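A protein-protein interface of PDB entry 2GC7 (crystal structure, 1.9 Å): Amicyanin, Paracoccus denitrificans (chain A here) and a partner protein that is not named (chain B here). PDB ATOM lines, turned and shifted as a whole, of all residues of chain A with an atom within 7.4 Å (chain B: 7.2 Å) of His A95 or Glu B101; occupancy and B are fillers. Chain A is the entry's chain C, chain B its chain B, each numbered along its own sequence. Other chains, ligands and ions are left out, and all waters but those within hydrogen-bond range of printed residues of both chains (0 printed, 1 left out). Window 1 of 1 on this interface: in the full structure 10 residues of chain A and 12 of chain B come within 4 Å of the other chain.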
ATOM      1  N   MET A  28       6.248 -18.069  -0.722  1.00  0.00           N
ATOM      2  CA  MET A  28       5.910 -16.730  -0.252  1.00  0.00           C
ATOM      3  C   MET A  28       4.586 -16.195  -0.785  1.00  0.00           C
ATOM      4  O   MET A  28       4.492 -15.018  -1.132  1.00  0.00           O
ATOM      5  CB  MET A  28       7.031 -15.743  -0.611  1.00  0.00           C
ATOM      6  CG  MET A  28       8.387 -16.078  -0.004  1.00  0.00           C
ATOM      7  SD  MET A  28       8.342 -16.186   1.798  1.00  0.00           S
ATOM      8  CE  MET A  28       8.432 -14.473   2.253  1.00  0.00           C
ATOM      9  N   TYR A  30      -0.086 -16.946  -0.909  1.00  0.00           N
ATOM     10  CA  TYR A  30      -1.294 -17.713  -0.647  1.00  0.00           C
ATOM     11  C   TYR A  30      -1.665 -18.122  -2.072  1.00  0.00           C
ATOM     12  O   TYR A  30      -1.990 -17.268  -2.892  1.00  0.00           O
ATOM     13  CB  TYR A  30      -2.366 -16.814  -0.027  1.00  0.00           C
ATOM     14  CG  TYR A  30      -1.969 -16.267   1.334  1.00  0.00           C
ATOM     15  CD1 TYR A  30      -1.777 -17.123   2.423  1.00  0.00           C
ATOM     16  CD2 TYR A  30      -1.757 -14.899   1.526  1.00  0.00           C
ATOM     17  CE1 TYR A  30      -1.381 -16.632   3.675  1.00  0.00           C
ATOM     18  CE2 TYR A  30      -1.362 -14.395   2.777  1.00  0.00           C
ATOM     19  CZ  TYR A  30      -1.178 -15.268   3.842  1.00  0.00           C
ATOM     20  OH  TYR A  30      -0.799 -14.778   5.075  1.00  0.00           O
ATOM     21  N   GLU A  49       5.598 -24.908   3.003  1.00  0.00           N
ATOM     22  CA  GLU A  49       7.046 -24.700   2.965  1.00  0.00           C
ATOM     23  C   GLU A  49       7.645 -24.487   4.358  1.00  0.00           C
ATOM     24  O   GLU A  49       6.931 -24.173   5.310  1.00  0.00           O
ATOM     25  CB  GLU A  49       7.389 -23.516   2.044  1.00  0.00           C
ATOM     26  CG  GLU A  49       6.863 -22.153   2.501  1.00  0.00           C
ATOM     27  CD  GLU A  49       7.203 -21.038   1.512  1.00  0.00           C
ATOM     28  OE1 GLU A  49       8.035 -21.278   0.608  1.00  0.00           O
ATOM     29  OE2 GLU A  49       6.649 -19.923   1.638  1.00  0.00           O
ATOM     30  N   MET A  51       9.512 -22.105   5.511  1.00  0.00           N
ATOM     31  CA  MET A  51       9.320 -20.724   5.952  1.00  0.00           C
ATOM     32  C   MET A  51       7.982 -20.565   6.684  1.00  0.00           C
ATOM     33  O   MET A  51       6.921 -20.745   6.088  1.00  0.00           O
ATOM     34  CB  MET A  51       9.339 -19.802   4.730  1.00  0.00           C
ATOM     35  CG  MET A  51       8.955 -18.365   5.005  1.00  0.00           C
ATOM     36  SD  MET A  51      10.286 -17.466   5.787  1.00  0.00           S
ATOM     37  CE  MET A  51      11.396 -17.234   4.390  1.00  0.00           C
ATOM     38  N   PRO A  52       8.012 -20.222   7.987  1.00  0.00           N
ATOM     39  CA  PRO A  52       6.768 -20.052   8.750  1.00  0.00           C
ATOM     40  C   PRO A  52       5.899 -18.899   8.251  1.00  0.00           C
ATOM     41  O   PRO A  52       6.416 -17.855   7.855  1.00  0.00           O
ATOM     42  CB  PRO A  52       7.268 -19.819  10.175  1.00  0.00           C
ATOM     43  CG  PRO A  52       8.568 -20.605  10.204  1.00  0.00           C
ATOM     44  CD  PRO A  52       9.181 -20.210   8.885  1.00  0.00           C
ATOM     45  N   HIS A  53       4.582 -19.098   8.281  1.00  0.00           N
ATOM     46  CA  HIS A  53       3.609 -18.087   7.843  1.00  0.00           C
ATOM     47  C   HIS A  53       2.365 -18.164   8.727  1.00  0.00           C
ATOM     48  O   HIS A  53       2.175 -19.122   9.469  1.00  0.00           O
ATOM     49  CB  HIS A  53       3.150 -18.331   6.401  1.00  0.00           C
ATOM     50  CG  HIS A  53       4.245 -18.294   5.381  1.00  0.00           C
ATOM     51  ND1 HIS A  53       4.965 -17.165   5.058  1.00  0.00           N
ATOM     52  CD2 HIS A  53       4.711 -19.274   4.565  1.00  0.00           C
ATOM     53  CE1 HIS A  53       5.819 -17.484   4.071  1.00  0.00           C
ATOM     54  NE2 HIS A  53       5.706 -18.755   3.736  1.00  0.00           N
ATOM     55  N   ASN A  54       1.506 -17.160   8.619  1.00  0.00           N
ATOM     56  CA  ASN A  54       0.270 -17.130   9.391  1.00  0.00           C
ATOM     57  C   ASN A  54      -0.710 -16.250   8.628  1.00  0.00           C
ATOM     58  O   ASN A  54      -0.397 -15.759   7.543  1.00  0.00           O
ATOM     59  CB  ASN A  54       0.528 -16.537  10.785  1.00  0.00           C
ATOM     60  CG  ASN A  54       0.645 -15.011  10.771  1.00  0.00           C
ATOM     61  OD1 ASN A  54       1.108 -14.414   9.798  1.00  0.00           O
ATOM     62  ND2 ASN A  54       0.230 -14.378  11.864  1.00  0.00           N
ATOM     63  N   MET A  71       1.600 -18.739  14.039  1.00  0.00           N
ATOM     64  CA  MET A  71       2.531 -19.052  12.963  1.00  0.00           C
ATOM     65  C   MET A  71       2.501 -20.547  12.673  1.00  0.00           C
ATOM     66  O   MET A  71       2.590 -21.372  13.586  1.00  0.00           O
ATOM     67  CB  MET A  71       3.953 -18.622  13.338  1.00  0.00           C
ATOM     68  CG  MET A  71       4.176 -17.114  13.341  1.00  0.00           C
ATOM     69  SD  MET A  71       3.979 -16.349  11.709  1.00  0.00           S
ATOM     70  CE  MET A  71       5.641 -16.520  11.047  1.00  0.00           C
ATOM     71  N   HIS A  91      -3.081 -10.727   5.669  1.00  0.00           N
ATOM     72  CA  HIS A  91      -1.686 -10.777   5.247  1.00  0.00           C
ATOM     73  C   HIS A  91      -0.915 -11.623   6.250  1.00  0.00           C
ATOM     74  O   HIS A  91      -1.474 -12.079   7.244  1.00  0.00           O
ATOM     75  CB  HIS A  91      -1.072  -9.368   5.195  1.00  0.00           C
ATOM     76  CG  HIS A  91      -0.887  -8.735   6.543  1.00  0.00           C
ATOM     77  ND1 HIS A  91      -1.930  -8.194   7.263  1.00  0.00           N
ATOM     78  CD2 HIS A  91       0.218  -8.585   7.314  1.00  0.00           C
ATOM     79  CE1 HIS A  91      -1.479  -7.740   8.419  1.00  0.00           C
ATOM     80  NE2 HIS A  91      -0.178  -7.965   8.475  1.00  0.00           N
ATOM     81  N   CYS A  92       0.368 -11.834   5.977  1.00  0.00           N
ATOM     82  CA  CYS A  92       1.229 -12.604   6.865  1.00  0.00           C
ATOM     83  C   CYS A  92       1.984 -11.591   7.727  1.00  0.00           C
ATOM     84  O   CYS A  92       2.655 -10.703   7.203  1.00  0.00           O
ATOM     85  CB  CYS A  92       2.209 -13.432   6.042  1.00  0.00           C
ATOM     86  SG  CYS A  92       3.252 -14.494   7.032  1.00  0.00           S
ATOM     87  N   THR A  93       1.876 -11.733   9.045  1.00  0.00           N
ATOM     88  CA  THR A  93       2.505 -10.800   9.977  1.00  0.00           C
ATOM     89  C   THR A  93       3.940 -10.358   9.653  1.00  0.00           C
ATOM     90  O   THR A  93       4.182  -9.173   9.450  1.00  0.00           O
ATOM     91  CB  THR A  93       2.432 -11.352  11.417  1.00  0.00           C
ATOM     92  OG1 THR A  93       1.055 -11.526  11.777  1.00  0.00           O
ATOM     93  CG2 THR A  93       3.089 -10.391  12.401  1.00  0.00           C
ATOM     94  N   PRO A  94       4.905 -11.292   9.595  1.00  0.00           N
ATOM     95  CA  PRO A  94       6.284 -10.883   9.286  1.00  0.00           C
ATOM     96  C   PRO A  94       6.539 -10.576   7.808  1.00  0.00           C
ATOM     97  O   PRO A  94       7.583 -10.024   7.453  1.00  0.00           O
ATOM     98  CB  PRO A  94       7.108 -12.074   9.764  1.00  0.00           C
ATOM     99  CG  PRO A  94       6.208 -13.226   9.444  1.00  0.00           C
ATOM    100  CD  PRO A  94       4.846 -12.732   9.906  1.00  0.00           C
ATOM    101  N   HIS A  95       5.585 -10.937   6.955  1.00  0.00           N
ATOM    102  CA  HIS A  95       5.709 -10.729   5.511  1.00  0.00           C
ATOM    103  C   HIS A  95       4.504  -9.932   5.016  1.00  0.00           C
ATOM    104  O   HIS A  95       3.632 -10.470   4.333  1.00  0.00           O
ATOM    105  CB  HIS A  95       5.755 -12.088   4.809  1.00  0.00           C
ATOM    106  CG  HIS A  95       6.655 -13.081   5.477  1.00  0.00           C
ATOM    107  ND1 HIS A  95       6.388 -14.430   5.567  1.00  0.00           N
ATOM    108  CD2 HIS A  95       7.856 -12.905   6.086  1.00  0.00           C
ATOM    109  CE1 HIS A  95       7.409 -15.012   6.212  1.00  0.00           C
ATOM    110  NE2 HIS A  95       8.327 -14.124   6.548  1.00  0.00           N
ATOM    111  N   PRO A  96       4.450  -8.630   5.349  1.00  0.00           N
ATOM    112  CA  PRO A  96       3.361  -7.720   4.966  1.00  0.00           C
ATOM    113  C   PRO A  96       3.025  -7.707   3.474  1.00  0.00           C
ATOM    114  O   PRO A  96       1.904  -7.374   3.088  1.00  0.00           O
ATOM    115  CB  PRO A  96       3.859  -6.357   5.454  1.00  0.00           C
ATOM    116  CG  PRO A  96       4.736  -6.719   6.621  1.00  0.00           C
ATOM    117  CD  PRO A  96       5.500  -7.903   6.083  1.00  0.00           C
ATOM    118  N   PHE A  97       3.998  -8.064   2.644  1.00  0.00           N
ATOM    119  CA  PHE A  97       3.795  -8.092   1.203  1.00  0.00           C
ATOM    120  C   PHE A  97       2.936  -9.270   0.748  1.00  0.00           C
ATOM    121  O   PHE A  97       2.455  -9.284  -0.386  1.00  0.00           O
ATOM    122  CB  PHE A  97       5.137  -8.139   0.476  1.00  0.00           C
ATOM    123  CG  PHE A  97       6.073  -9.177   1.011  1.00  0.00           C
ATOM    124  CD1 PHE A  97       6.795  -8.945   2.177  1.00  0.00           C
ATOM    125  CD2 PHE A  97       6.218 -10.400   0.365  1.00  0.00           C
ATOM    126  CE1 PHE A  97       7.646  -9.920   2.693  1.00  0.00           C
ATOM    127  CE2 PHE A  97       7.065 -11.380   0.872  1.00  0.00           C
ATOM    128  CZ  PHE A  97       7.780 -11.139   2.039  1.00  0.00           C
ATOM    129  N   MET A  98       2.763 -10.264   1.617  1.00  0.00           N
ATOM    130  CA  MET A  98       1.933 -11.430   1.294  1.00  0.00           C
ATOM    131  C   MET A  98       0.494 -11.085   1.640  1.00  0.00           C
ATOM    132  O   MET A  98       0.164 -10.902   2.813  1.00  0.00           O
ATOM    133  CB  MET A  98       2.339 -12.643   2.125  1.00  0.00           C
ATOM    134  CG  MET A  98       3.498 -13.426   1.595  1.00  0.00           C
ATOM    135  SD  MET A  98       3.909 -14.754   2.741  1.00  0.00           S
ATOM    136  CE  MET A  98       2.583 -15.956   2.407  1.00  0.00           C
ATOM    137  N   ARG A  99      -0.360 -11.011   0.628  1.00  0.00           N
ATOM    138  CA  ARG A  99      -1.757 -10.662   0.843  1.00  0.00           C
ATOM    139  C   ARG A  99      -2.727 -11.690   0.271  1.00  0.00           C
ATOM    140  O   ARG A  99      -2.462 -12.326  -0.749  1.00  0.00           O
ATOM    141  CB  ARG A  99      -2.062  -9.304   0.213  1.00  0.00           C
ATOM    142  CG  ARG A  99      -2.452  -8.220   1.204  1.00  0.00           C
ATOM    143  CD  ARG A  99      -1.261  -7.395   1.639  1.00  0.00           C
ATOM    144  NE  ARG A  99      -0.536  -6.872   0.486  1.00  0.00           N
ATOM    145  CZ  ARG A  99       0.412  -5.943   0.553  1.00  0.00           C
ATOM    146  NH1 ARG A  99       1.021  -5.539  -0.554  1.00  0.00           N
ATOM    147  NH2 ARG A  99       0.743  -5.405   1.721  1.00  0.00           N
ATOM    148  N   ALA B  55       6.334 -14.165  15.429  1.00  0.00           N
ATOM    149  CA  ALA B  55       6.895 -13.851  14.117  1.00  0.00           C
ATOM    150  C   ALA B  55       8.394 -13.598  14.216  1.00  0.00           C
ATOM    151  O   ALA B  55       8.884 -13.144  15.250  1.00  0.00           O
ATOM    152  CB  ALA B  55       6.198 -12.630  13.534  1.00  0.00           C
ATOM    153  N   SER B  56       9.126 -13.889  13.144  1.00  0.00           N
ATOM    154  CA  SER B  56      10.568 -13.670  13.151  1.00  0.00           C
ATOM    155  C   SER B  56      11.199 -13.755  11.770  1.00  0.00           C
ATOM    156  O   SER B  56      10.552 -14.120  10.790  1.00  0.00           O
ATOM    157  CB  SER B  56      11.255 -14.705  14.037  1.00  0.00           C
ATOM    158  OG  SER B  56      11.282 -15.960  13.382  1.00  0.00           O
ATOM    159  N   TRQ B  57      12.479 -13.404  11.713  1.00  0.00           N
ATOM    160  CA  TRQ B  57      13.234 -13.488  10.485  1.00  0.00           C
ATOM    161  C   TRQ B  57      13.827 -14.894  10.546  1.00  0.00           C
ATOM    162  O   TRQ B  57      13.856 -15.506  11.616  1.00  0.00           O
ATOM    163  CB  TRQ B  57      14.321 -12.401  10.455  1.00  0.00           C
ATOM    164  CG  TRQ B  57      15.435 -12.549  11.465  1.00  0.00           C
ATOM    165  CD1 TRQ B  57      16.569 -13.298  11.301  1.00  0.00           C
ATOM    166  NE1 TRQ B  57      17.374 -13.199  12.403  1.00  0.00           N
ATOM    167  CE2 TRQ B  57      16.774 -12.377  13.318  1.00  0.00           C
ATOM    168  CZ2 TRQ B  57      17.231 -11.997  14.591  1.00  0.00           C
ATOM    169  CH2 TRQ B  57      16.440 -11.155  15.327  1.00  0.00           C
ATOM    170  CZ3 TRQ B  57      15.211 -10.687  14.836  1.00  0.00           C
ATOM    171  CE3 TRQ B  57      14.746 -11.060  13.570  1.00  0.00           C
ATOM    172  CD2 TRQ B  57      15.536 -11.932  12.778  1.00  0.00           C
ATOM    173  O6  TRQ B  57      16.833 -10.820  16.463  1.00  0.00           O
ATOM    174  O7  TRQ B  57      18.327 -12.448  14.976  1.00  0.00           O
ATOM    175  N   VAL B  58      14.262 -15.430   9.412  1.00  0.00           N
ATOM    176  CA  VAL B  58      14.838 -16.772   9.404  1.00  0.00           C
ATOM    177  C   VAL B  58      16.157 -16.787   8.656  1.00  0.00           C
ATOM    178  O   VAL B  58      16.553 -15.797   8.040  1.00  0.00           O
ATOM    179  CB  VAL B  58      13.895 -17.808   8.723  1.00  0.00           C
ATOM    180  CG1 VAL B  58      12.557 -17.865   9.449  1.00  0.00           C
ATOM    181  CG2 VAL B  58      13.690 -17.438   7.259  1.00  0.00           C
ATOM    182  N   ALA B  59      16.839 -17.923   8.721  1.00  0.00           N
ATOM    183  CA  ALA B  59      18.098 -18.104   8.024  1.00  0.00           C
ATOM    184  C   ALA B  59      18.362 -19.590   7.874  1.00  0.00           C
ATOM    185  O   ALA B  59      17.954 -20.392   8.711  1.00  0.00           O
ATOM    186  CB  ALA B  59      19.230 -17.448   8.794  1.00  0.00           C
ATOM    187  N   LEU B  95      19.684 -10.490   4.372  1.00  0.00           N
ATOM    188  CA  LEU B  95      19.360  -9.524   3.321  1.00  0.00           C
ATOM    189  C   LEU B  95      18.895  -8.177   3.888  1.00  0.00           C
ATOM    190  O   LEU B  95      18.575  -8.072   5.072  1.00  0.00           O
ATOM    191  CB  LEU B  95      18.278 -10.117   2.414  1.00  0.00           C
ATOM    192  CG  LEU B  95      18.730 -10.994   1.236  1.00  0.00           C
ATOM    193  CD1 LEU B  95      19.958 -11.786   1.585  1.00  0.00           C
ATOM    194  CD2 LEU B  95      17.589 -11.903   0.817  1.00  0.00           C
ATOM    195  N   PRO B  96      18.861  -7.126   3.045  1.00  0.00           N
ATOM    196  CA  PRO B  96      18.435  -5.790   3.472  1.00  0.00           C
ATOM    197  C   PRO B  96      16.995  -5.773   3.982  1.00  0.00           C
ATOM    198  O   PRO B  96      16.244  -6.731   3.789  1.00  0.00           O
ATOM    199  CB  PRO B  96      18.625  -4.941   2.210  1.00  0.00           C
ATOM    200  CG  PRO B  96      19.744  -5.634   1.501  1.00  0.00           C
ATOM    201  CD  PRO B  96      19.362  -7.090   1.659  1.00  0.00           C
ATOM    202  N   VAL B  97      16.615  -4.675   4.627  1.00  0.00           N
ATOM    203  CA  VAL B  97      15.280  -4.543   5.206  1.00  0.00           C
ATOM    204  C   VAL B  97      14.103  -4.718   4.235  1.00  0.00           C
ATOM    205  O   VAL B  97      13.006  -5.076   4.664  1.00  0.00           O
ATOM    206  CB  VAL B  97      15.133  -3.179   5.946  1.00  0.00           C
ATOM    207  CG1 VAL B  97      14.954  -2.044   4.939  1.00  0.00           C
ATOM    208  CG2 VAL B  97      13.963  -3.234   6.919  1.00  0.00           C
ATOM    209  N   TYR B  98      14.312  -4.483   2.939  1.00  0.00           N
ATOM    210  CA  TYR B  98      13.214  -4.632   1.982  1.00  0.00           C
ATOM    211  C   TYR B  98      12.930  -6.103   1.645  1.00  0.00           C
ATOM    212  O   TYR B  98      12.079  -6.413   0.814  1.00  0.00           O
ATOM    213  CB  TYR B  98      13.468  -3.794   0.715  1.00  0.00           C
ATOM    214  CG  TYR B  98      14.706  -4.145  -0.077  1.00  0.00           C
ATOM    215  CD1 TYR B  98      14.654  -5.079  -1.115  1.00  0.00           C
ATOM    216  CD2 TYR B  98      15.930  -3.533   0.197  1.00  0.00           C
ATOM    217  CE1 TYR B  98      15.790  -5.392  -1.862  1.00  0.00           C
ATOM    218  CE2 TYR B  98      17.075  -3.841  -0.545  1.00  0.00           C
ATOM    219  CZ  TYR B  98      16.995  -4.771  -1.572  1.00  0.00           C
ATOM    220  OH  TYR B  98      18.119  -5.085  -2.300  1.00  0.00           O
ATOM    221  N   ARG B  99      13.655  -6.999   2.311  1.00  0.00           N
ATOM    222  CA  ARG B  99      13.475  -8.450   2.187  1.00  0.00           C
ATOM    223  C   ARG B  99      13.450  -8.858   3.659  1.00  0.00           C
ATOM    224  O   ARG B  99      14.302  -9.616   4.129  1.00  0.00           O
ATOM    225  CB  ARG B  99      14.665  -9.105   1.475  1.00  0.00           C
ATOM    226  CG  ARG B  99      14.795  -8.778  -0.019  1.00  0.00           C
ATOM    227  CD  ARG B  99      13.604  -9.308  -0.814  1.00  0.00           C
ATOM    228  NE  ARG B  99      13.476 -10.759  -0.695  1.00  0.00           N
ATOM    229  CZ  ARG B  99      14.280 -11.637  -1.287  1.00  0.00           C
ATOM    230  NH1 ARG B  99      14.083 -12.937  -1.110  1.00  0.00           N
ATOM    231  NH2 ARG B  99      15.272 -11.216  -2.067  1.00  0.00           N
ATOM    232  N   PRO B 100      12.457  -8.348   4.406  1.00  0.00           N
ATOM    233  CA  PRO B 100      12.278  -8.601   5.836  1.00  0.00           C
ATOM    234  C   PRO B 100      12.315 -10.046   6.294  1.00  0.00           C
ATOM    235  O   PRO B 100      12.765 -10.324   7.402  1.00  0.00           O
ATOM    236  CB  PRO B 100      10.951  -7.908   6.144  1.00  0.00           C
ATOM    237  CG  PRO B 100      10.207  -8.039   4.871  1.00  0.00           C
ATOM    238  CD  PRO B 100      11.251  -7.711   3.843  1.00  0.00           C
ATOM    239  N   GLU B 101      11.853 -10.966   5.451  1.00  0.00           N
ATOM    240  CA  GLU B 101      11.854 -12.373   5.823  1.00  0.00           C
ATOM    241  C   GLU B 101      13.257 -12.843   6.235  1.00  0.00           C
ATOM    242  O   GLU B 101      13.389 -13.786   7.015  1.00  0.00           O
ATOM    243  CB  GLU B 101      11.322 -13.241   4.666  1.00  0.00           C
ATOM    244  CG  GLU B 101      12.148 -13.177   3.381  1.00  0.00           C
ATOM    245  CD  GLU B 101      11.637 -12.138   2.389  1.00  0.00           C
ATOM    246  OE1 GLU B 101      11.182 -11.056   2.826  1.00  0.00           O
ATOM    247  OE2 GLU B 101      11.702 -12.400   1.164  1.00  0.00           O
ATOM    248  N   PHE B 102      14.297 -12.185   5.721  1.00  0.00           N
ATOM    249  CA  PHE B 102      15.682 -12.551   6.046  1.00  0.00           C
ATOM    250  C   PHE B 102      16.490 -11.417   6.695  1.00  0.00           C
ATOM    251  O   PHE B 102      17.716 -11.510   6.779  1.00  0.00           O
ATOM    252  CB  PHE B 102      16.442 -12.981   4.785  1.00  0.00           C
ATOM    253  CG  PHE B 102      15.874 -14.192   4.101  1.00  0.00           C
ATOM    254  CD1 PHE B 102      15.850 -15.427   4.746  1.00  0.00           C
ATOM    255  CD2 PHE B 102      15.383 -14.103   2.802  1.00  0.00           C
ATOM    256  CE1 PHE B 102      15.345 -16.560   4.103  1.00  0.00           C
ATOM    257  CE2 PHE B 102      14.873 -15.232   2.148  1.00  0.00           C
ATOM    258  CZ  PHE B 102      14.857 -16.460   2.803  1.00  0.00           C
ATOM    259  N   ALA B 103      15.820 -10.361   7.149  1.00  0.00           N
ATOM    260  CA  ALA B 103      16.514  -9.208   7.745  1.00  0.00           C
ATOM    261  C   ALA B 103      16.617  -9.316   9.259  1.00  0.00           C
ATOM    262  O   ALA B 103      15.604  -9.554   9.918  1.00  0.00           O
ATOM    263  CB  ALA B 103      15.780  -7.928   7.368  1.00  0.00           C
ATOM    264  N   ASN B 104      17.812  -9.119   9.828  1.00  0.00           N
ATOM    265  CA  ASN B 104      17.923  -9.246  11.280  1.00  0.00           C
ATOM    266  C   ASN B 104      18.171  -8.015  12.167  1.00  0.00           C
ATOM    267  O   ASN B 104      18.500  -8.166  13.343  1.00  0.00           O
ATOM    268  CB  ASN B 104      18.890 -10.401  11.647  1.00  0.00           C
ATOM    269  CG  ASN B 104      20.376 -10.054  11.484  1.00  0.00           C
ATOM    270  OD1 ASN B 104      21.229 -10.948  11.549  1.00  0.00           O
ATOM    271  ND2 ASN B 104      20.693  -8.781  11.293  1.00  0.00           N
ATOM    272  N   ILE B 106      15.746  -5.913  12.487  1.00  0.00           N
ATOM    273  CA  ILE B 106      14.371  -5.731  12.935  1.00  0.00           C
ATOM    274  C   ILE B 106      14.150  -6.411  14.278  1.00  0.00           C
ATOM    275  O   ILE B 106      14.668  -7.501  14.518  1.00  0.00           O
ATOM    276  CB  ILE B 106      13.377  -6.334  11.908  1.00  0.00           C
ATOM    277  CG1 ILE B 106      13.452  -5.557  10.593  1.00  0.00           C
ATOM    278  CG2 ILE B 106      11.950  -6.304  12.464  1.00  0.00           C
ATOM    279  CD1 ILE B 106      12.654  -6.186   9.469  1.00  0.00           C
ATOM    280  N   TRP B 108      12.224  -8.611  16.136  1.00  0.00           N
ATOM    281  CA  TRP B 108      11.211  -9.619  15.860  1.00  0.00           C
ATOM    282  C   TRP B 108      10.446 -10.024  17.118  1.00  0.00           C
ATOM    283  O   TRP B 108      10.586 -11.140  17.614  1.00  0.00           O
ATOM    284  CB  TRP B 108      11.873 -10.833  15.176  1.00  0.00           C
ATOM    285  CG  TRP B 108      12.230 -10.553  13.719  1.00  0.00           C
ATOM    286  CD1 TRP B 108      13.483 -10.606  13.116  1.00  0.00           C
ATOM    287  CD2 TRP B 108      11.320 -10.112  12.704  1.00  0.00           C
ATOM    288  NE1 TRP B 108      13.381 -10.207  11.807  1.00  0.00           N
ATOM    289  CE2 TRP B 108      12.072  -9.905  11.526  1.00  0.00           C
ATOM    290  CE3 TRP B 108       9.935  -9.873  12.678  1.00  0.00           C
ATOM    291  CZ2 TRP B 108      11.485  -9.471  10.330  1.00  0.00           C
ATOM    292  CZ3 TRP B 108       9.353  -9.443  11.489  1.00  0.00           C
ATOM    293  CH2 TRP B 108      10.129  -9.248  10.332  1.00  0.00           C
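Of the printed residues of chain B, Met A28 touches Glu B101 (3.96 Å). Glu A49 touches none of the printed residues of chain B. Of the printed residues of chain B, Met A51 touches Val B58 and Phe B102. Of chain B, only Glu B101 (3.6 Å) comes within 4 Å of His A95. Of the printed residues of chain A, Ala B55 touches Thr A93 (3.995 Å) and Pro A94 (3.9 Å). Printed residues of chain A within 4 Å of Phe B102: Met A51. Of the printed residues of chain A, Trp B108 touches Pro A94 (3.9 Å). The nearest residue of chain B that does not touch His A95 is Ser B56 (4.8 Å). The nearest printed residue of chain A that does not touch Glu B101 is Met A51 (4.003 Å). The nearest printed residue of chain A that does not touch Pro B100 is Pro A94 (4.2 Å).
The guanidinium group (NE) of Arg B99 is in salt-bridge range of the side-chain carboxylate (OE2) of Glu B101 (3.0 Å). CE3 of TRQ B57 is covalently linked to CD1 of Trp B108. The backbone carbonyl oxygen of Ala B103 is in hydrogen-bond range of NE1 of Trp B108 (3.0 Å). N of Met A28 sits at hydrogen-bond distance from OE2 of Glu A49 (3.0 Å). N of Leu B95 is in hydrogen-bond range of O of Phe B102. SG of Cys A92 lies within hydrogen-bond range of ND1 of His A95.
Of the 17 printed residues of chain A, 6 touch a printed residue of chain B. Printed residues of chain A that touch a printed residue of chain B: Met A28, Met A51, Thr A93, Pro A94, His A95 and Phe A97. Hydrophobic or aromatic side chains of chain B that line the printed part of chain A: Ala B55, Val B58, Pro B100, Phe B102 and Trp B108. Among the printed residues, 9 pairs touch across the chains.
Met A28 touches Glu B101. Val B58 touches Met A51. Phe B102 touches Met A51. Ala B55 touches Thr A93. Ala B55 touches Pro A94 (CB to CD, 3.9 Å). Pro A94 touches Trp B108. Glu B101 touches His A95 (CB to NE2, 3.6 Å). CE1 of Phe A97 touches CG of Pro B100, 3.9 Å away. CZ of Phe A97 touches OE1 of Glu B101, 3.5 Å away.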
